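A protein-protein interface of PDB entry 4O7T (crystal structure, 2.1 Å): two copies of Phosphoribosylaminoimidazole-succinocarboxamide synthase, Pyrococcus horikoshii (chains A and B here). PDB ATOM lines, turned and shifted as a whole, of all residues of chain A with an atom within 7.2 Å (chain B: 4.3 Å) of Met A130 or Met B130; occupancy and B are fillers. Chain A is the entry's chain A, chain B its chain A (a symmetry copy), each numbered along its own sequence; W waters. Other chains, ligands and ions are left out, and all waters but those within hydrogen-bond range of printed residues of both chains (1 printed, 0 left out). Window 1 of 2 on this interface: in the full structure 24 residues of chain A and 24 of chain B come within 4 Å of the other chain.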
ATOM      1  N   SER A  99     -20.883   3.603  28.719  1.00  0.00           N
ATOM      2  CA  SER A  99     -20.953   2.223  28.201  1.00  0.00           C
ATOM      3  C   SER A  99     -21.864   2.061  26.978  1.00  0.00           C
ATOM      4  O   SER A  99     -21.717   1.095  26.210  1.00  0.00           O
ATOM      5  CB  SER A  99     -21.397   1.244  29.300  1.00  0.00           C
ATOM      6  OG  SER A  99     -22.766   1.455  29.608  1.00  0.00           O
ATOM      7  N   LYS A 102     -20.448   1.196  23.564  1.00  0.00           N
ATOM      8  CA  LYS A 102     -20.137  -0.216  23.290  1.00  0.00           C
ATOM      9  C   LYS A 102     -21.349  -1.035  22.816  1.00  0.00           C
ATOM     10  O   LYS A 102     -21.201  -2.178  22.386  1.00  0.00           O
ATOM     11  CB  LYS A 102     -19.538  -0.902  24.529  1.00  0.00           C
ATOM     12  CG  LYS A 102     -18.272  -0.272  25.083  1.00  0.00           C
ATOM     13  CD  LYS A 102     -17.783  -1.068  26.292  1.00  0.00           C
ATOM     14  N   ARG A 103     -22.548  -0.476  22.887  1.00  0.00           N
ATOM     15  CA  ARG A 103     -23.725  -1.238  22.454  1.00  0.00           C
ATOM     16  C   ARG A 103     -24.314  -0.756  21.150  1.00  0.00           C
ATOM     17  O   ARG A 103     -24.987  -1.524  20.468  1.00  0.00           O
ATOM     18  CB  ARG A 103     -24.816  -1.225  23.520  1.00  0.00           C
ATOM     19  CG  ARG A 103     -24.620  -2.289  24.566  1.00  0.00           C
ATOM     20  CD  ARG A 103     -25.571  -2.122  25.724  1.00  0.00           C
ATOM     21  NE  ARG A 103     -24.869  -2.425  26.962  1.00  0.00           N
ATOM     22  CZ  ARG A 103     -24.402  -3.635  27.279  1.00  0.00           C
ATOM     23  NH1 ARG A 103     -24.555  -4.686  26.458  1.00  0.00           N
ATOM     24  NH2 ARG A 103     -23.770  -3.791  28.429  1.00  0.00           N
ATOM     25  N   VAL A 117     -33.874   2.606  28.384  1.00  0.00           N
ATOM     26  CA  VAL A 117     -33.827   2.109  29.768  1.00  0.00           C
ATOM     27  C   VAL A 117     -33.022   0.823  29.747  1.00  0.00           C
ATOM     28  O   VAL A 117     -33.282  -0.059  28.928  1.00  0.00           O
ATOM     29  CB  VAL A 117     -35.236   1.841  30.357  1.00  0.00           C
ATOM     30  CG1 VAL A 117     -35.142   1.493  31.837  1.00  0.00           C
ATOM     31  CG2 VAL A 117     -36.125   3.068  30.179  1.00  0.00           C
ATOM     32  N   GLU A 118     -32.019   0.740  30.611  1.00  0.00           N
ATOM     33  CA  GLU A 118     -31.201  -0.468  30.760  1.00  0.00           C
ATOM     34  C   GLU A 118     -31.330  -1.006  32.193  1.00  0.00           C
ATOM     35  O   GLU A 118     -31.401  -0.231  33.150  1.00  0.00           O
ATOM     36  CB  GLU A 118     -29.724  -0.173  30.454  1.00  0.00           C
ATOM     37  CG  GLU A 118     -29.459   0.375  29.047  1.00  0.00           C
ATOM     38  CD  GLU A 118     -27.998   0.758  28.814  1.00  0.00           C
ATOM     39  OE1 GLU A 118     -27.251   0.995  29.800  1.00  0.00           O
ATOM     40  OE2 GLU A 118     -27.583   0.837  27.630  1.00  0.00           O
ATOM     41  N   LEU A 119     -31.375  -2.326  32.322  1.00  0.00           N
ATOM     42  CA  LEU A 119     -31.403  -2.985  33.620  1.00  0.00           C
ATOM     43  C   LEU A 119     -30.062  -3.646  33.878  1.00  0.00           C
ATOM     44  O   LEU A 119     -29.533  -4.344  32.998  1.00  0.00           O
ATOM     45  CB  LEU A 119     -32.507  -4.043  33.669  1.00  0.00           C
ATOM     46  CG  LEU A 119     -33.919  -3.540  33.355  1.00  0.00           C
ATOM     47  CD1 LEU A 119     -34.882  -4.710  33.188  1.00  0.00           C
ATOM     48  CD2 LEU A 119     -34.401  -2.558  34.426  1.00  0.00           C
ATOM     49  N   TYR A 120     -29.523  -3.425  35.076  1.00  0.00           N
ATOM     50  CA  TYR A 120     -28.298  -4.087  35.516  1.00  0.00           C
ATOM     51  C   TYR A 120     -28.556  -4.833  36.810  1.00  0.00           C
ATOM     52  O   TYR A 120     -29.195  -4.314  37.723  1.00  0.00           O
ATOM     53  CB  TYR A 120     -27.178  -3.075  35.727  1.00  0.00           C
ATOM     54  CG  TYR A 120     -26.714  -2.445  34.437  1.00  0.00           C
ATOM     55  CD1 TYR A 120     -25.674  -3.014  33.700  1.00  0.00           C
ATOM     56  CD2 TYR A 120     -27.329  -1.291  33.947  1.00  0.00           C
ATOM     57  CE1 TYR A 120     -25.242  -2.433  32.515  1.00  0.00           C
ATOM     58  CE2 TYR A 120     -26.913  -0.705  32.755  1.00  0.00           C
ATOM     59  CZ  TYR A 120     -25.867  -1.275  32.047  1.00  0.00           C
ATOM     60  OH  TYR A 120     -25.453  -0.684  30.867  1.00  0.00           O
ATOM     61  N   TYR A 121     -28.065  -6.058  36.876  1.00  0.00           N
ATOM     62  CA  TYR A 121     -28.227  -6.879  38.059  1.00  0.00           C
ATOM     63  C   TYR A 121     -27.135  -6.496  39.072  1.00  0.00           C
ATOM     64  O   TYR A 121     -25.949  -6.594  38.774  1.00  0.00           O
ATOM     65  CB  TYR A 121     -28.156  -8.350  37.651  1.00  0.00           C
ATOM     66  CG  TYR A 121     -28.111  -9.359  38.794  1.00  0.00           C
ATOM     67  CD1 TYR A 121     -28.847  -9.160  39.965  1.00  0.00           C
ATOM     68  CD2 TYR A 121     -27.353 -10.531  38.681  1.00  0.00           C
ATOM     69  CE1 TYR A 121     -28.830 -10.095  40.993  1.00  0.00           C
ATOM     70  CE2 TYR A 121     -27.329 -11.468  39.709  1.00  0.00           C
ATOM     71  CZ  TYR A 121     -28.063 -11.233  40.855  1.00  0.00           C
ATOM     72  OH  TYR A 121     -28.050 -12.136  41.863  1.00  0.00           O
ATOM     73  N   LEU A 126     -20.492 -10.921  39.900  1.00  0.00           N
ATOM     74  CA  LEU A 126     -20.661 -10.818  38.449  1.00  0.00           C
ATOM     75  C   LEU A 126     -20.386  -9.424  37.880  1.00  0.00           C
ATOM     76  O   LEU A 126     -20.488  -9.210  36.672  1.00  0.00           O
ATOM     77  CB  LEU A 126     -22.065 -11.315  38.045  1.00  0.00           C
ATOM     78  CG  LEU A 126     -22.417 -12.754  38.448  1.00  0.00           C
ATOM     79  CD1 LEU A 126     -23.839 -13.110  38.037  1.00  0.00           C
ATOM     80  CD2 LEU A 126     -21.422 -13.757  37.868  1.00  0.00           C
ATOM     81  N   HIS A 127     -20.020  -8.484  38.744  1.00  0.00           N
ATOM     82  CA  HIS A 127     -19.722  -7.100  38.331  1.00  0.00           C
ATOM     83  C   HIS A 127     -20.868  -6.430  37.622  1.00  0.00           C
ATOM     84  O   HIS A 127     -20.687  -5.840  36.559  1.00  0.00           O
ATOM     85  CB  HIS A 127     -18.452  -7.029  37.470  1.00  0.00           C
ATOM     86  CG  HIS A 127     -17.293  -7.804  38.039  1.00  0.00           C
ATOM     87  ND1 HIS A 127     -16.625  -7.404  39.145  1.00  0.00           N
ATOM     88  CD2 HIS A 127     -16.692  -8.996  37.622  1.00  0.00           C
ATOM     89  CE1 HIS A 127     -15.648  -8.293  39.425  1.00  0.00           C
ATOM     90  NE2 HIS A 127     -15.691  -9.268  38.490  1.00  0.00           N
ATOM     91  N   ASP A 128     -22.059  -6.515  38.217  1.00  0.00           N
ATOM     92  CA  ASP A 128     -23.236  -5.776  37.754  1.00  0.00           C
ATOM     93  C   ASP A 128     -23.552  -5.938  36.256  1.00  0.00           C
ATOM     94  O   ASP A 128     -23.557  -4.956  35.511  1.00  0.00           O
ATOM     95  CB  ASP A 128     -23.112  -4.303  38.140  1.00  0.00           C
ATOM     96  CG  ASP A 128     -22.984  -4.103  39.646  1.00  0.00           C
ATOM     97  OD1 ASP A 128     -23.349  -5.000  40.424  1.00  0.00           O
ATOM     98  OD2 ASP A 128     -22.510  -3.042  40.067  1.00  0.00           O
ATOM     99  N   PRO A 129     -23.819  -7.184  35.811  1.00  0.00           N
ATOM    100  CA  PRO A 129     -24.030  -7.376  34.371  1.00  0.00           C
ATOM    101  C   PRO A 129     -25.386  -6.824  33.926  1.00  0.00           C
ATOM    102  O   PRO A 129     -26.347  -6.799  34.720  1.00  0.00           O
ATOM    103  CB  PRO A 129     -24.008  -8.898  34.220  1.00  0.00           C
ATOM    104  CG  PRO A 129     -24.541  -9.402  35.518  1.00  0.00           C
ATOM    105  CD  PRO A 129     -23.977  -8.450  36.557  1.00  0.00           C
ATOM    106  N   MET A 130     -25.454  -6.373  32.674  1.00  0.00           N
ATOM    107  CA  MET A 130     -26.741  -6.018  32.082  1.00  0.00           C
ATOM    108  C   MET A 130     -27.644  -7.248  31.997  1.00  0.00           C
ATOM    109  O   MET A 130     -27.180  -8.361  31.709  1.00  0.00           O
ATOM    110  CB  MET A 130     -26.576  -5.373  30.705  1.00  0.00           C
ATOM    111  CG  MET A 130     -27.756  -4.468  30.358  1.00  0.00           C
ATOM    112  SD  MET A 130     -27.709  -3.665  28.735  1.00  0.00           S
ATOM    113  CE  MET A 130     -28.045  -5.069  27.690  1.00  0.00           C
ATOM    114  N   ILE A 131     -28.925  -7.050  32.274  1.00  0.00           N
ATOM    115  CA  ILE A 131     -29.900  -8.110  32.116  1.00  0.00           C
ATOM    116  C   ILE A 131     -31.116  -7.584  31.380  1.00  0.00           C
ATOM    117  O   ILE A 131     -31.252  -6.367  31.175  1.00  0.00           O
ATOM    118  CB  ILE A 131     -30.359  -8.710  33.469  1.00  0.00           C
ATOM    119  CG1 ILE A 131     -30.901  -7.614  34.406  1.00  0.00           C
ATOM    120  CG2 ILE A 131     -29.236  -9.540  34.090  1.00  0.00           C
ATOM    121  CD1 ILE A 131     -31.772  -8.140  35.539  1.00  0.00           C
ATOM    122  N   ASN A 132     -31.993  -8.505  30.990  1.00  0.00           N
ATOM    123  CA  ASN A 132     -33.310  -8.133  30.456  1.00  0.00           C
ATOM    124  C   ASN A 132     -34.462  -8.647  31.361  1.00  0.00           C
ATOM    125  O   ASN A 132     -34.225  -9.162  32.474  1.00  0.00           O
ATOM    126  CB  ASN A 132     -33.448  -8.562  28.976  1.00  0.00           C
ATOM    127  CG  ASN A 132     -33.433 -10.075  28.792  1.00  0.00           C
ATOM    128  OD1 ASN A 132     -33.936 -10.824  29.634  1.00  0.00           O
ATOM    129  ND2 ASN A 132     -32.857 -10.530  27.688  1.00  0.00           N
ATOM    130  N   HIS A 135     -34.194 -12.489  32.470  1.00  0.00           N
ATOM    131  CA  HIS A 135     -33.261 -12.739  33.563  1.00  0.00           C
ATOM    132  C   HIS A 135     -33.901 -12.249  34.844  1.00  0.00           C
ATOM    133  O   HIS A 135     -33.846 -12.926  35.867  1.00  0.00           O
ATOM    134  CB  HIS A 135     -31.932 -12.013  33.380  1.00  0.00           C
ATOM    135  CG  HIS A 135     -31.293 -12.174  32.014  1.00  0.00           C
ATOM    136  ND1 HIS A 135     -30.652 -13.295  31.636  1.00  0.00           N
ATOM    137  CD2 HIS A 135     -31.142 -11.277  30.976  1.00  0.00           C
ATOM    138  CE1 HIS A 135     -30.161 -13.129  30.395  1.00  0.00           C
ATOM    139  NE2 HIS A 135     -30.449 -11.894  30.001  1.00  0.00           N
ATOM    140  N   ARG B 103     -24.227 -13.875  33.759  1.00  0.00           N
ATOM    141  CA  ARG B 103     -25.328 -12.947  34.045  1.00  0.00           C
ATOM    142  C   ARG B 103     -26.143 -13.327  35.257  1.00  0.00           C
ATOM    143  O   ARG B 103     -26.780 -12.463  35.854  1.00  0.00           O
ATOM    144  CB  ARG B 103     -26.264 -12.812  32.847  1.00  0.00           C
ATOM    145  CG  ARG B 103     -25.784 -11.797  31.846  1.00  0.00           C
ATOM    146  CD  ARG B 103     -26.593 -11.836  30.573  1.00  0.00           C
ATOM    147  NE  ARG B 103     -25.701 -11.649  29.438  1.00  0.00           N
ATOM    148  CZ  ARG B 103     -25.028 -10.523  29.195  1.00  0.00           C
ATOM    149  NH1 ARG B 103     -25.132  -9.453  30.000  1.00  0.00           N
ATOM    150  NH2 ARG B 103     -24.237 -10.470  28.137  1.00  0.00           N
ATOM    151  N   LEU B 119     -31.412 -10.858  23.287  1.00  0.00           N
ATOM    152  CA  LEU B 119     -31.177 -10.214  22.003  1.00  0.00           C
ATOM    153  C   LEU B 119     -29.733  -9.756  21.925  1.00  0.00           C
ATOM    154  O   LEU B 119     -29.226  -9.134  22.872  1.00  0.00           O
ATOM    155  CB  LEU B 119     -32.102  -9.009  21.822  1.00  0.00           C
ATOM    156  CG  LEU B 119     -33.600  -9.300  21.948  1.00  0.00           C
ATOM    157  CD1 LEU B 119     -34.397  -8.002  22.000  1.00  0.00           C
ATOM    158  CD2 LEU B 119     -34.077 -10.212  20.815  1.00  0.00           C
ATOM    159  N   TYR B 120     -29.082 -10.065  20.804  1.00  0.00           N
ATOM    160  CA  TYR B 120     -27.729  -9.590  20.530  1.00  0.00           C
ATOM    161  C   TYR B 120     -27.708  -8.827  19.221  1.00  0.00           C
ATOM    162  O   TYR B 120     -28.293  -9.257  18.230  1.00  0.00           O
ATOM    163  CB  TYR B 120     -26.749 -10.754  20.456  1.00  0.00           C
ATOM    164  CG  TYR B 120     -26.550 -11.433  21.788  1.00  0.00           C
ATOM    165  CD1 TYR B 120     -25.542 -11.013  22.658  1.00  0.00           C
ATOM    166  CD2 TYR B 120     -27.382 -12.481  22.185  1.00  0.00           C
ATOM    167  CE1 TYR B 120     -25.353 -11.639  23.883  1.00  0.00           C
ATOM    168  CE2 TYR B 120     -27.212 -13.111  23.415  1.00  0.00           C
ATOM    169  CZ  TYR B 120     -26.194 -12.690  24.257  1.00  0.00           C
ATOM    170  OH  TYR B 120     -26.024 -13.325  25.475  1.00  0.00           O
ATOM    171  N   ASP B 128     -20.910  -8.113  18.676  1.00  0.00           N
ATOM    172  CA  ASP B 128     -22.231  -8.670  18.977  1.00  0.00           C
ATOM    173  C   ASP B 128     -22.710  -8.450  20.423  1.00  0.00           C
ATOM    174  O   ASP B 128     -22.952  -9.414  21.152  1.00  0.00           O
ATOM    175  CB  ASP B 128     -22.272 -10.149  18.596  1.00  0.00           C
ATOM    176  CG  ASP B 128     -21.982 -10.379  17.117  1.00  0.00           C
ATOM    177  OD1 ASP B 128     -22.111  -9.447  16.307  1.00  0.00           O
ATOM    178  OD2 ASP B 128     -21.616 -11.502  16.750  1.00  0.00           O
ATOM    179  N   PRO B 129     -22.849  -7.174  20.842  1.00  0.00           N
ATOM    180  CA  PRO B 129     -23.213  -6.940  22.245  1.00  0.00           C
ATOM    181  C   PRO B 129     -24.680  -7.287  22.507  1.00  0.00           C
ATOM    182  O   PRO B 129     -25.524  -7.180  21.596  1.00  0.00           O
ATOM    183  CB  PRO B 129     -22.992  -5.436  22.411  1.00  0.00           C
ATOM    184  CG  PRO B 129     -23.275  -4.873  21.061  1.00  0.00           C
ATOM    185  CD  PRO B 129     -22.726  -5.906  20.093  1.00  0.00           C
ATOM    186  N   MET B 130     -24.973  -7.712  23.736  1.00  0.00           N
ATOM    187  CA  MET B 130     -26.362  -7.872  24.155  1.00  0.00           C
ATOM    188  C   MET B 130     -27.082  -6.524  24.134  1.00  0.00           C
ATOM    189  O   MET B 130     -26.503  -5.486  24.490  1.00  0.00           O
ATOM    190  CB  MET B 130     -26.471  -8.521  25.535  1.00  0.00           C
ATOM    191  CG  MET B 130     -27.803  -9.243  25.719  1.00  0.00           C
ATOM    192  SD  MET B 130     -28.081 -10.030  27.328  1.00  0.00           S
ATOM    193  CE  MET B 130     -28.343  -8.582  28.334  1.00  0.00           C
ATOM    194  N   ILE B 131     -28.332  -6.537  23.693  1.00  0.00           N
ATOM    195  CA  ILE B 131     -29.157  -5.347  23.735  1.00  0.00           C
ATOM    196  C   ILE B 131     -30.519  -5.685  24.304  1.00  0.00           C
ATOM    197  O   ILE B 131     -30.855  -6.867  24.479  1.00  0.00           O
ATOM    198  CB  ILE B 131     -29.347  -4.699  22.340  1.00  0.00           C
ATOM    199  CG1 ILE B 131     -29.916  -5.714  21.331  1.00  0.00           C
ATOM    200  CG2 ILE B 131     -28.045  -4.045  21.876  1.00  0.00           C
ATOM    201  CD1 ILE B 131     -30.549  -5.079  20.100  1.00  0.00           C
ATOM    202  N   HIS B 135     -32.692  -0.397  22.874  1.00  0.00           N
ATOM    203  CA  HIS B 135     -31.600  -0.295  21.912  1.00  0.00           C
ATOM    204  C   HIS B 135     -32.135  -0.699  20.555  1.00  0.00           C
ATOM    205  O   HIS B 135     -31.852  -0.046  19.554  1.00  0.00           O
ATOM    206  CB  HIS B 135     -30.425  -1.203  22.257  1.00  0.00           C
ATOM    207  CG  HIS B 135     -29.950  -1.123  23.695  1.00  0.00           C
ATOM    208  ND1 HIS B 135     -29.207  -0.103  24.163  1.00  0.00           N
ATOM    209  CD2 HIS B 135     -30.064  -2.023  24.735  1.00  0.00           C
ATOM    210  CE1 HIS B 135     -28.908  -0.326  25.455  1.00  0.00           C
ATOM    211  NE2 HIS B 135     -29.420  -1.503  25.798  1.00  0.00           N
HETATM  212  O   HOH W   1     -31.626  -9.178  25.594  1.00  0.00           O
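Water W1 lies within hydrogen-bond range of O of Ile B131 (2.7 Å), ND2 of Asn A132 (2.8 Å) and N of Leu B119 (2.9 Å).
CG of Pro B129 touches O of Lys A102 (3.6 Å). Pro B129 touches Arg A103 (CG to O, 3.8 Å). Arg A103 touches His B135. CD2 of Tyr A121 touches O of Arg B103 (3.5 Å). C of Arg B103 touches CD1 of Leu A126, 3.6 Å away. Pro A129 touches Arg B103 (CG to O, 3.8 Å). Met A130 touches Met B130. CE1 of His A135 touches CD of Arg B103, at 3.8 Å.
Met A130 touches just these residues of chain B: Arg B103 (2.9 Å) and Met B130 (3.6 Å). Of chain A, only Arg A103 (2.9 Å) and Met A130 (3.6 Å) come within 4 Å of Met B130. Printed residues of chain B within 4 Å of Tyr A121: Arg B103. Printed residues of chain B within 4 Å of Lys A102: Pro B129 (3.6 Å). The nearest residue of chain B that does not touch Met A130 is His B135 (4.03 Å). The nearest printed residue of chain B that does not touch His A135 is Met B130 (4.03 Å).
NE of Arg A103 is in hydrogen-bond range of SD of Met A130 (3.6 Å). OE1 of Glu A118 lies within hydrogen-bond range of OH of Tyr A120 (2.7 Å). N of Tyr A121 sits at hydrogen-bond distance from O of Pro A129. The side-chain amide oxygen of Asn A132 lies close to the backbone NH of His A135, 3.3 Å away. NE of Arg B103 is in hydrogen-bond range of SD of Met B130, at 3.6 Å.
Arg A103 touches Pro B129, and with the chains exchanged Pro A129 touches Arg B103. Arg A103 touches Met B130, and with the chains exchanged Met A130 touches Arg B103. Arg A103 touches His B135, and with the chains exchanged His A135 touches Arg B103. Met B130 touches its own counterpart, Met A130. 8 positions are printed for both chains.
The backbone carbonyl oxygen (O) of Met B130 lies within hydrogen-bond range of the guanidinium group (NH1) of Arg A103 (2.9 Å). A ring nitrogen (NE2) of His B135 lies close to the side-chain carboxylate (OE2) of Glu A118. O of Met A130 sits at hydrogen-bond distance from NH1 of Arg B103, 2.9 Å away.
Along chain B the printed residues that touch a printed residue of chain A span positions 103 to 135. Among the printed residues, no Asp or Glu carboxylate lies within 4 Å of a Lys or Arg side-chain nitrogen of the other chain.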
